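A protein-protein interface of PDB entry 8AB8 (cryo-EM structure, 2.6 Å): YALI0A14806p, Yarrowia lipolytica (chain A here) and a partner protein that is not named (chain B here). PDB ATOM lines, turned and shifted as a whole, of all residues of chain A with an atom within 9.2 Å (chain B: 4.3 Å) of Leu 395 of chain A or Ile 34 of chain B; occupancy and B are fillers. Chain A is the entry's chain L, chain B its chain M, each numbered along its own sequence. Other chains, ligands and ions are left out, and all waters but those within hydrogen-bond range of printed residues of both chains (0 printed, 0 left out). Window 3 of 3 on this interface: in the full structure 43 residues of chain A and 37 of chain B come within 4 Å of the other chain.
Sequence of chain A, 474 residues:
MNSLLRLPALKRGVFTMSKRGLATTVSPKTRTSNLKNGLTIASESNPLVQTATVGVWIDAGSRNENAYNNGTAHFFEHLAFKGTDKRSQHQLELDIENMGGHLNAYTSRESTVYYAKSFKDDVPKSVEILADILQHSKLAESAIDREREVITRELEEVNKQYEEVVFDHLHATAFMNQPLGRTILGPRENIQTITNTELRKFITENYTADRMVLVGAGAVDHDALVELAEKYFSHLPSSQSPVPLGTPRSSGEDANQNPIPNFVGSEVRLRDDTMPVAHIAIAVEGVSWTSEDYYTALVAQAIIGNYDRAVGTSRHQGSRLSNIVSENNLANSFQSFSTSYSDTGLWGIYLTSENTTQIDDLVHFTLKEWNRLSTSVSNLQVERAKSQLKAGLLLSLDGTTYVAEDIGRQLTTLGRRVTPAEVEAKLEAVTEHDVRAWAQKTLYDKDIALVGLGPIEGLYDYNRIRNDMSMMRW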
ATOM      1  N   VAL A  26      29.997   7.695   3.082  1.00  0.00           N
ATOM      2  CA  VAL A  26      30.411   7.598   1.638  1.00  0.00           C
ATOM      3  C   VAL A  26      30.502   6.130   1.221  1.00  0.00           C
ATOM      4  O   VAL A  26      31.372   5.384   1.676  1.00  0.00           O
ATOM      5  CB  VAL A  26      31.715   8.375   1.345  1.00  0.00           C
ATOM      6  CG1 VAL A  26      32.162   8.258  -0.113  1.00  0.00           C
ATOM      7  CG2 VAL A  26      31.605   9.839   1.749  1.00  0.00           C
ATOM      8  N   SER A  27      29.623   5.759   0.283  1.00  0.00           N
ATOM      9  CA  SER A  27      29.550   4.429  -0.298  1.00  0.00           C
ATOM     10  C   SER A  27      30.780   4.144  -1.163  1.00  0.00           C
ATOM     11  O   SER A  27      31.362   5.075  -1.721  1.00  0.00           O
ATOM     12  CB  SER A  27      28.282   4.311  -1.093  1.00  0.00           C
ATOM     13  OG  SER A  27      28.042   2.962  -1.450  1.00  0.00           O
ATOM     14  N   LEU A  48      30.373  -6.022   3.730  1.00  0.00           N
ATOM     15  CA  LEU A  48      29.557  -6.195   4.924  1.00  0.00           C
ATOM     16  C   LEU A  48      28.460  -7.236   4.701  1.00  0.00           C
ATOM     17  O   LEU A  48      27.903  -7.752   5.669  1.00  0.00           O
ATOM     18  CB  LEU A  48      28.940  -4.849   5.317  1.00  0.00           C
ATOM     19  CG  LEU A  48      29.475  -4.170   6.581  1.00  0.00           C
ATOM     20  CD1 LEU A  48      28.326  -3.615   7.408  1.00  0.00           C
ATOM     21  CD2 LEU A  48      30.349  -5.085   7.431  1.00  0.00           C
ATOM     22  N   SER A 387      15.550  18.952   1.355  1.00  0.00           N
ATOM     23  CA  SER A 387      16.058  18.247   2.523  1.00  0.00           C
ATOM     24  C   SER A 387      15.606  16.792   2.516  1.00  0.00           C
ATOM     25  O   SER A 387      16.418  15.889   2.682  1.00  0.00           O
ATOM     26  CB  SER A 387      15.644  18.935   3.785  1.00  0.00           C
ATOM     27  OG  SER A 387      16.342  20.160   3.907  1.00  0.00           O
ATOM     28  N   GLN A 388      14.316  16.592   2.253  1.00  0.00           N
ATOM     29  CA  GLN A 388      13.661  15.302   2.193  1.00  0.00           C
ATOM     30  C   GLN A 388      14.242  14.414   1.089  1.00  0.00           C
ATOM     31  O   GLN A 388      14.199  13.192   1.229  1.00  0.00           O
ATOM     32  CB  GLN A 388      12.176  15.569   1.964  1.00  0.00           C
ATOM     33  CG  GLN A 388      11.293  14.338   2.049  1.00  0.00           C
ATOM     34  CD  GLN A 388       9.934  14.678   2.613  1.00  0.00           C
ATOM     35  OE1 GLN A 388       9.378  15.748   2.364  1.00  0.00           O
ATOM     36  NE2 GLN A 388       9.384  13.756   3.389  1.00  0.00           N
ATOM     37  N   LEU A 389      14.722  15.019  -0.010  1.00  0.00           N
ATOM     38  CA  LEU A 389      15.119  14.281  -1.207  1.00  0.00           C
ATOM     39  C   LEU A 389      16.592  13.894  -1.142  1.00  0.00           C
ATOM     40  O   LEU A 389      16.990  12.837  -1.639  1.00  0.00           O
ATOM     41  CB  LEU A 389      14.888  15.146  -2.450  1.00  0.00           C
ATOM     42  CG  LEU A 389      13.575  14.964  -3.207  1.00  0.00           C
ATOM     43  CD1 LEU A 389      13.550  15.914  -4.395  1.00  0.00           C
ATOM     44  CD2 LEU A 389      13.400  13.530  -3.691  1.00  0.00           C
ATOM     45  N   LYS A 390      17.394  14.789  -0.560  1.00  0.00           N
ATOM     46  CA  LYS A 390      18.812  14.554  -0.385  1.00  0.00           C
ATOM     47  C   LYS A 390      19.024  13.234   0.357  1.00  0.00           C
ATOM     48  O   LYS A 390      19.927  12.479   0.004  1.00  0.00           O
ATOM     49  CB  LYS A 390      19.489  15.820   0.155  1.00  0.00           C
ATOM     50  CG  LYS A 390      20.479  15.620   1.293  1.00  0.00           C
ATOM     51  CD  LYS A 390      21.858  15.206   0.815  1.00  0.00           C
ATOM     52  CE  LYS A 390      22.812  14.836   1.930  1.00  0.00           C
ATOM     53  NZ  LYS A 390      24.217  14.813   1.456  1.00  0.00           N
ATOM     54  N   ALA A 391      18.161  12.930   1.333  1.00  0.00           N
ATOM     55  CA  ALA A 391      18.194  11.640   2.008  1.00  0.00           C
ATOM     56  C   ALA A 391      17.488  10.562   1.186  1.00  0.00           C
ATOM     57  O   ALA A 391      17.985   9.443   1.085  1.00  0.00           O
ATOM     58  CB  ALA A 391      17.616  11.752   3.395  1.00  0.00           C
ATOM     59  N   GLY A 392      16.326  10.899   0.615  1.00  0.00           N
ATOM     60  CA  GLY A 392      15.451   9.924  -0.021  1.00  0.00           C
ATOM     61  C   GLY A 392      16.127   9.172  -1.164  1.00  0.00           C
ATOM     62  O   GLY A 392      15.880   7.987  -1.362  1.00  0.00           O
ATOM     63  N   LEU A 393      16.983   9.882  -1.906  1.00  0.00           N
ATOM     64  CA  LEU A 393      17.658   9.333  -3.070  1.00  0.00           C
ATOM     65  C   LEU A 393      18.758   8.356  -2.655  1.00  0.00           C
ATOM     66  O   LEU A 393      19.210   7.549  -3.463  1.00  0.00           O
ATOM     67  CB  LEU A 393      18.196  10.495  -3.915  1.00  0.00           C
ATOM     68  CG  LEU A 393      17.129  11.300  -4.659  1.00  0.00           C
ATOM     69  CD1 LEU A 393      17.702  12.594  -5.202  1.00  0.00           C
ATOM     70  CD2 LEU A 393      16.505  10.484  -5.782  1.00  0.00           C
ATOM     71  N   LEU A 394      19.200   8.454  -1.399  1.00  0.00           N
ATOM     72  CA  LEU A 394      20.216   7.568  -0.856  1.00  0.00           C
ATOM     73  C   LEU A 394      19.571   6.405  -0.106  1.00  0.00           C
ATOM     74  O   LEU A 394      20.101   5.296  -0.160  1.00  0.00           O
ATOM     75  CB  LEU A 394      21.156   8.383   0.040  1.00  0.00           C
ATOM     76  CG  LEU A 394      21.870   9.544  -0.655  1.00  0.00           C
ATOM     77  CD1 LEU A 394      22.709  10.340   0.331  1.00  0.00           C
ATOM     78  CD2 LEU A 394      22.722   9.069  -1.828  1.00  0.00           C
ATOM     79  N   LEU A 395      18.442   6.676   0.584  1.00  0.00           N
ATOM     80  CA  LEU A 395      17.785   5.735   1.484  1.00  0.00           C
ATOM     81  C   LEU A 395      17.205   4.557   0.711  1.00  0.00           C
ATOM     82  O   LEU A 395      17.112   3.449   1.241  1.00  0.00           O
ATOM     83  CB  LEU A 395      16.679   6.449   2.274  1.00  0.00           C
ATOM     84  CG  LEU A 395      16.955   6.672   3.763  1.00  0.00           C
ATOM     85  CD1 LEU A 395      17.872   7.858   3.998  1.00  0.00           C
ATOM     86  CD2 LEU A 395      15.657   6.877   4.522  1.00  0.00           C
ATOM     87  N   SER A 396      16.730   4.836  -0.503  1.00  0.00           N
ATOM     88  CA  SER A 396      16.151   3.837  -1.387  1.00  0.00           C
ATOM     89  C   SER A 396      17.100   2.655  -1.592  1.00  0.00           C
ATOM     90  O   SER A 396      16.646   1.519  -1.715  1.00  0.00           O
ATOM     91  CB  SER A 396      15.716   4.459  -2.688  1.00  0.00           C
ATOM     92  OG  SER A 396      16.606   5.493  -3.074  1.00  0.00           O
ATOM     93  N   LEU A 397      18.412   2.920  -1.607  1.00  0.00           N
ATOM     94  CA  LEU A 397      19.412   1.902  -1.903  1.00  0.00           C
ATOM     95  C   LEU A 397      19.809   1.174  -0.625  1.00  0.00           C
ATOM     96  O   LEU A 397      20.806   1.507   0.010  1.00  0.00           O
ATOM     97  CB  LEU A 397      20.638   2.577  -2.525  1.00  0.00           C
ATOM     98  CG  LEU A 397      20.386   3.859  -3.309  1.00  0.00           C
ATOM     99  CD1 LEU A 397      21.707   4.537  -3.618  1.00  0.00           C
ATOM    100  CD2 LEU A 397      19.669   3.573  -4.623  1.00  0.00           C
ATOM    101  N   ASP A 398      19.014   0.157  -0.266  1.00  0.00           N
ATOM    102  CA  ASP A 398      19.173  -0.607   0.958  1.00  0.00           C
ATOM    103  C   ASP A 398      20.012  -1.864   0.716  1.00  0.00           C
ATOM    104  O   ASP A 398      21.191  -1.908   1.069  1.00  0.00           O
ATOM    105  CB  ASP A 398      17.800  -0.999   1.506  1.00  0.00           C
ATOM    106  CG  ASP A 398      16.898   0.174   1.855  1.00  0.00           C
ATOM    107  OD1 ASP A 398      17.222   0.918   2.810  1.00  0.00           O
ATOM    108  OD2 ASP A 398      15.887   0.350   1.158  1.00  0.00           O
ATOM    109  N   GLY A 399      19.376  -2.886   0.130  1.00  0.00           N
ATOM    110  CA  GLY A 399      19.982  -4.182  -0.114  1.00  0.00           C
ATOM    111  C   GLY A 399      20.637  -4.241  -1.491  1.00  0.00           C
ATOM    112  O   GLY A 399      20.565  -3.290  -2.273  1.00  0.00           O
ATOM    113  N   TYR A 402      18.571  -3.548  -4.638  1.00  0.00           N
ATOM    114  CA  TYR A 402      18.253  -2.150  -4.874  1.00  0.00           C
ATOM    115  C   TYR A 402      19.460  -1.420  -5.452  1.00  0.00           C
ATOM    116  O   TYR A 402      19.312  -0.565  -6.325  1.00  0.00           O
ATOM    117  CB  TYR A 402      17.757  -1.474  -3.599  1.00  0.00           C
ATOM    118  CG  TYR A 402      16.447  -2.016  -3.102  1.00  0.00           C
ATOM    119  CD1 TYR A 402      15.312  -2.008  -3.904  1.00  0.00           C
ATOM    120  CD2 TYR A 402      16.344  -2.550  -1.828  1.00  0.00           C
ATOM    121  CE1 TYR A 402      14.103  -2.510  -3.443  1.00  0.00           C
ATOM    122  CE2 TYR A 402      15.144  -3.054  -1.352  1.00  0.00           C
ATOM    123  CZ  TYR A 402      14.019  -3.036  -2.163  1.00  0.00           C
ATOM    124  OH  TYR A 402      12.836  -3.534  -1.697  1.00  0.00           O
ATOM    125  N   VAL A 403      20.646  -1.779  -4.953  1.00  0.00           N
ATOM    126  CA  VAL A 403      21.870  -1.181  -5.446  1.00  0.00           C
ATOM    127  C   VAL A 403      22.075  -1.600  -6.898  1.00  0.00           C
ATOM    128  O   VAL A 403      22.422  -0.766  -7.727  1.00  0.00           O
ATOM    129  CB  VAL A 403      23.092  -1.517  -4.575  1.00  0.00           C
ATOM    130  CG1 VAL A 403      24.378  -0.984  -5.187  1.00  0.00           C
ATOM    131  CG2 VAL A 403      22.931  -0.982  -3.166  1.00  0.00           C
ATOM    132  N   SER B  32      28.474   3.467   4.043  1.00  0.00           N
ATOM    133  CA  SER B  32      27.268   3.892   3.356  1.00  0.00           C
ATOM    134  C   SER B  32      26.783   5.169   4.024  1.00  0.00           C
ATOM    135  O   SER B  32      27.090   5.383   5.193  1.00  0.00           O
ATOM    136  CB  SER B  32      26.222   2.799   3.388  1.00  0.00           C
ATOM    137  OG  SER B  32      25.133   3.147   4.202  1.00  0.00           O
ATOM    138  N   PRO B  33      26.021   6.051   3.341  1.00  0.00           N
ATOM    139  CA  PRO B  33      25.508   7.249   3.996  1.00  0.00           C
ATOM    140  C   PRO B  33      24.269   7.028   4.863  1.00  0.00           C
ATOM    141  O   PRO B  33      23.860   7.951   5.562  1.00  0.00           O
ATOM    142  CB  PRO B  33      25.190   8.190   2.831  1.00  0.00           C
ATOM    143  CG  PRO B  33      24.826   7.249   1.709  1.00  0.00           C
ATOM    144  CD  PRO B  33      25.683   6.015   1.911  1.00  0.00           C
ATOM    145  N   ILE B  34      23.711   5.805   4.854  1.00  0.00           N
ATOM    146  CA  ILE B  34      22.456   5.549   5.545  1.00  0.00           C
ATOM    147  C   ILE B  34      22.662   4.609   6.732  1.00  0.00           C
ATOM    148  O   ILE B  34      23.197   3.516   6.602  1.00  0.00           O
ATOM    149  CB  ILE B  34      21.324   5.093   4.593  1.00  0.00           C
ATOM    150  CG1 ILE B  34      21.743   3.935   3.675  1.00  0.00           C
ATOM    151  CG2 ILE B  34      20.788   6.289   3.811  1.00  0.00           C
ATOM    152  CD1 ILE B  34      20.602   3.121   3.074  1.00  0.00           C
ATOM    153  N   SER B  35      22.159   5.038   7.892  1.00  0.00           N
ATOM    154  CA  SER B  35      22.209   4.261   9.117  1.00  0.00           C
ATOM    155  C   SER B  35      20.806   3.787   9.481  1.00  0.00           C
ATOM    156  O   SER B  35      19.827   4.468   9.189  1.00  0.00           O
ATOM    157  CB  SER B  35      22.774   5.109  10.214  1.00  0.00           C
ATOM    158  OG  SER B  35      24.130   5.450   9.942  1.00  0.00           O
ATOM    159  N   GLY B  81      14.805  13.848   6.355  1.00  0.00           N
ATOM    160  CA  GLY B  81      14.444  12.818   5.400  1.00  0.00           C
ATOM    161  C   GLY B  81      14.514  11.410   5.988  1.00  0.00           C
ATOM    162  O   GLY B  81      14.655  10.445   5.244  1.00  0.00           O
ATOM    163  N   LYS B  83      13.131   7.915   7.987  1.00  0.00           N
ATOM    164  CA  LYS B  83      11.938   7.091   7.896  1.00  0.00           C
ATOM    165  C   LYS B  83      11.805   6.299   9.185  1.00  0.00           C
ATOM    166  O   LYS B  83      12.801   6.015   9.848  1.00  0.00           O
ATOM    167  CB  LYS B  83      12.057   6.022   6.813  1.00  0.00           C
ATOM    168  CG  LYS B  83      12.363   6.475   5.398  1.00  0.00           C
ATOM    169  CD  LYS B  83      11.201   7.116   4.673  1.00  0.00           C
ATOM    170  CE  LYS B  83      11.010   6.609   3.253  1.00  0.00           C
ATOM    171  NZ  LYS B  83      12.262   6.091   2.643  1.00  0.00           N
ATOM    172  N   GLN B  98      15.545   5.003   9.919  1.00  0.00           N
ATOM    173  CA  GLN B  98      16.545   5.005   8.877  1.00  0.00           C
ATOM    174  C   GLN B  98      16.854   6.463   8.570  1.00  0.00           C
ATOM    175  O   GLN B  98      15.931   7.241   8.377  1.00  0.00           O
ATOM    176  CB  GLN B  98      15.944   4.261   7.696  1.00  0.00           C
ATOM    177  CG  GLN B  98      16.928   3.987   6.582  1.00  0.00           C
ATOM    178  CD  GLN B  98      16.334   3.003   5.608  1.00  0.00           C
ATOM    179  OE1 GLN B  98      15.340   3.278   4.932  1.00  0.00           O
ATOM    180  NE2 GLN B  98      16.947   1.835   5.529  1.00  0.00           N
ATOM    181  N   PHE B  99      18.135   6.843   8.559  1.00  0.00           N
ATOM    182  CA  PHE B  99      18.478   8.250   8.412  1.00  0.00           C
ATOM    183  C   PHE B  99      19.877   8.355   7.822  1.00  0.00           C
ATOM    184  O   PHE B  99      20.540   7.349   7.629  1.00  0.00           O
ATOM    185  CB  PHE B  99      18.369   8.967   9.765  1.00  0.00           C
ATOM    186  CG  PHE B  99      19.020   8.213  10.897  1.00  0.00           C
ATOM    187  CD1 PHE B  99      18.312   7.231  11.579  1.00  0.00           C
ATOM    188  CD2 PHE B  99      20.347   8.445  11.248  1.00  0.00           C
ATOM    189  CE1 PHE B  99      18.915   6.493  12.589  1.00  0.00           C
ATOM    190  CE2 PHE B  99      20.953   7.703  12.257  1.00  0.00           C
ATOM    191  CZ  PHE B  99      20.235   6.731  12.925  1.00  0.00           C
ATOM    192  N   LEU B 100      20.343   9.586   7.598  1.00  0.00           N
ATOM    193  CA  LEU B 100      21.722   9.815   7.193  1.00  0.00           C
ATOM    194  C   LEU B 100      22.631   9.693   8.412  1.00  0.00           C
ATOM    195  O   LEU B 100      22.234  10.083   9.500  1.00  0.00           O
ATOM    196  CB  LEU B 100      21.834  11.206   6.570  1.00  0.00           C
ATOM    197  CG  LEU B 100      21.014  11.423   5.299  1.00  0.00           C
ATOM    198  CD1 LEU B 100      21.211  12.820   4.750  1.00  0.00           C
ATOM    199  CD2 LEU B 100      21.331  10.388   4.225  1.00  0.00           C
ATOM    200  N   ASN B 197      25.343   0.275  10.337  1.00  0.00           N
ATOM    201  CA  ASN B 197      26.137   1.333   9.707  1.00  0.00           C
ATOM    202  C   ASN B 197      26.231   2.525  10.662  1.00  0.00           C
ATOM    203  O   ASN B 197      26.092   3.684  10.272  1.00  0.00           O
ATOM    204  CB  ASN B 197      25.759   1.588   8.234  1.00  0.00           C
ATOM    205  CG  ASN B 197      26.492   2.732   7.556  1.00  0.00           C
ATOM    206  OD1 ASN B 197      27.697   2.684   7.320  1.00  0.00           O
ATOM    207  ND2 ASN B 197      25.756   3.781   7.219  1.00  0.00           N
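The side-chain carboxylate (OD1) of Asp 398 of chain A sits at hydrogen-bond distance from the side-chain amide nitrogen (NE2) of Gln 98 of chain B (2.9 Å).
The backbone NH of Ile 34 of chain B is in hydrogen-bond range of the side-chain hydroxyl of Ser 32 of chain B (3.1 Å). The side-chain amide nitrogen of Asn 197 of chain B sits at hydrogen-bond distance from the backbone carbonyl oxygen of Ile 34 of chain B (2.6 Å). N of Lys 83 of chain B lies within hydrogen-bond range of O of Gln 98 of chain B, 2.9 Å away.
Among the printed residues, merely in contact across the chains: Lys 390 of chain A with Leu 100 of chain B (3.8 Å), Ala 391 of chain A with Gly 81 of chain B (3.7 Å), Ala 391 of chain A with Leu 100 of chain B (3.9 Å), Leu 394 of chain A with Pro 33 of chain B (3.99 Å), Leu 394 of chain A with Ile 34 of chain B (3.9 Å), Leu 395 of chain A with Ile 34 of chain B (3.3 Å), Leu 395 of chain A with Gly 81 of chain B (3.8 Å), Leu 395 of chain A with Lys 83 of chain B (3.4 Å), Leu 395 of chain A with Gln 98 of chain B (3.6 Å) and Leu 397 of chain A with Ile 34 of chain B (3.5 Å).
Of the printed residues of chain B, Ala 391 of chain A touches Gly 81 and Leu 100. Printed residues of chain B within 4 Å of Asp 398 of chain A: Gln 98 (2.9 Å). Val 403 of chain A touches none of the printed residues of chain B. Ile 34 of chain B touches three residues of chain A. Ser 35 of chain B touches none of the printed residues of chain A. The nearest printed residue of chain B that does not touch Leu 395 of chain A is Leu 100 of chain B (4.3 Å). The nearest residue of chain A that does not touch Ile 34 of chain B is Asp 398 of chain A (4.04 Å).
Of the 10 printed residues of chain B, 6 touch a printed residue of chain A. Hydrophobic or aromatic side chains of chain B within 4 Å of the printed part of chain A: Pro 33, Ile 34 and Leu 100. Among the printed residues, no Asp or Glu carboxylate lies within 4 Å of a Lys or Arg side-chain nitrogen of the other chain.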
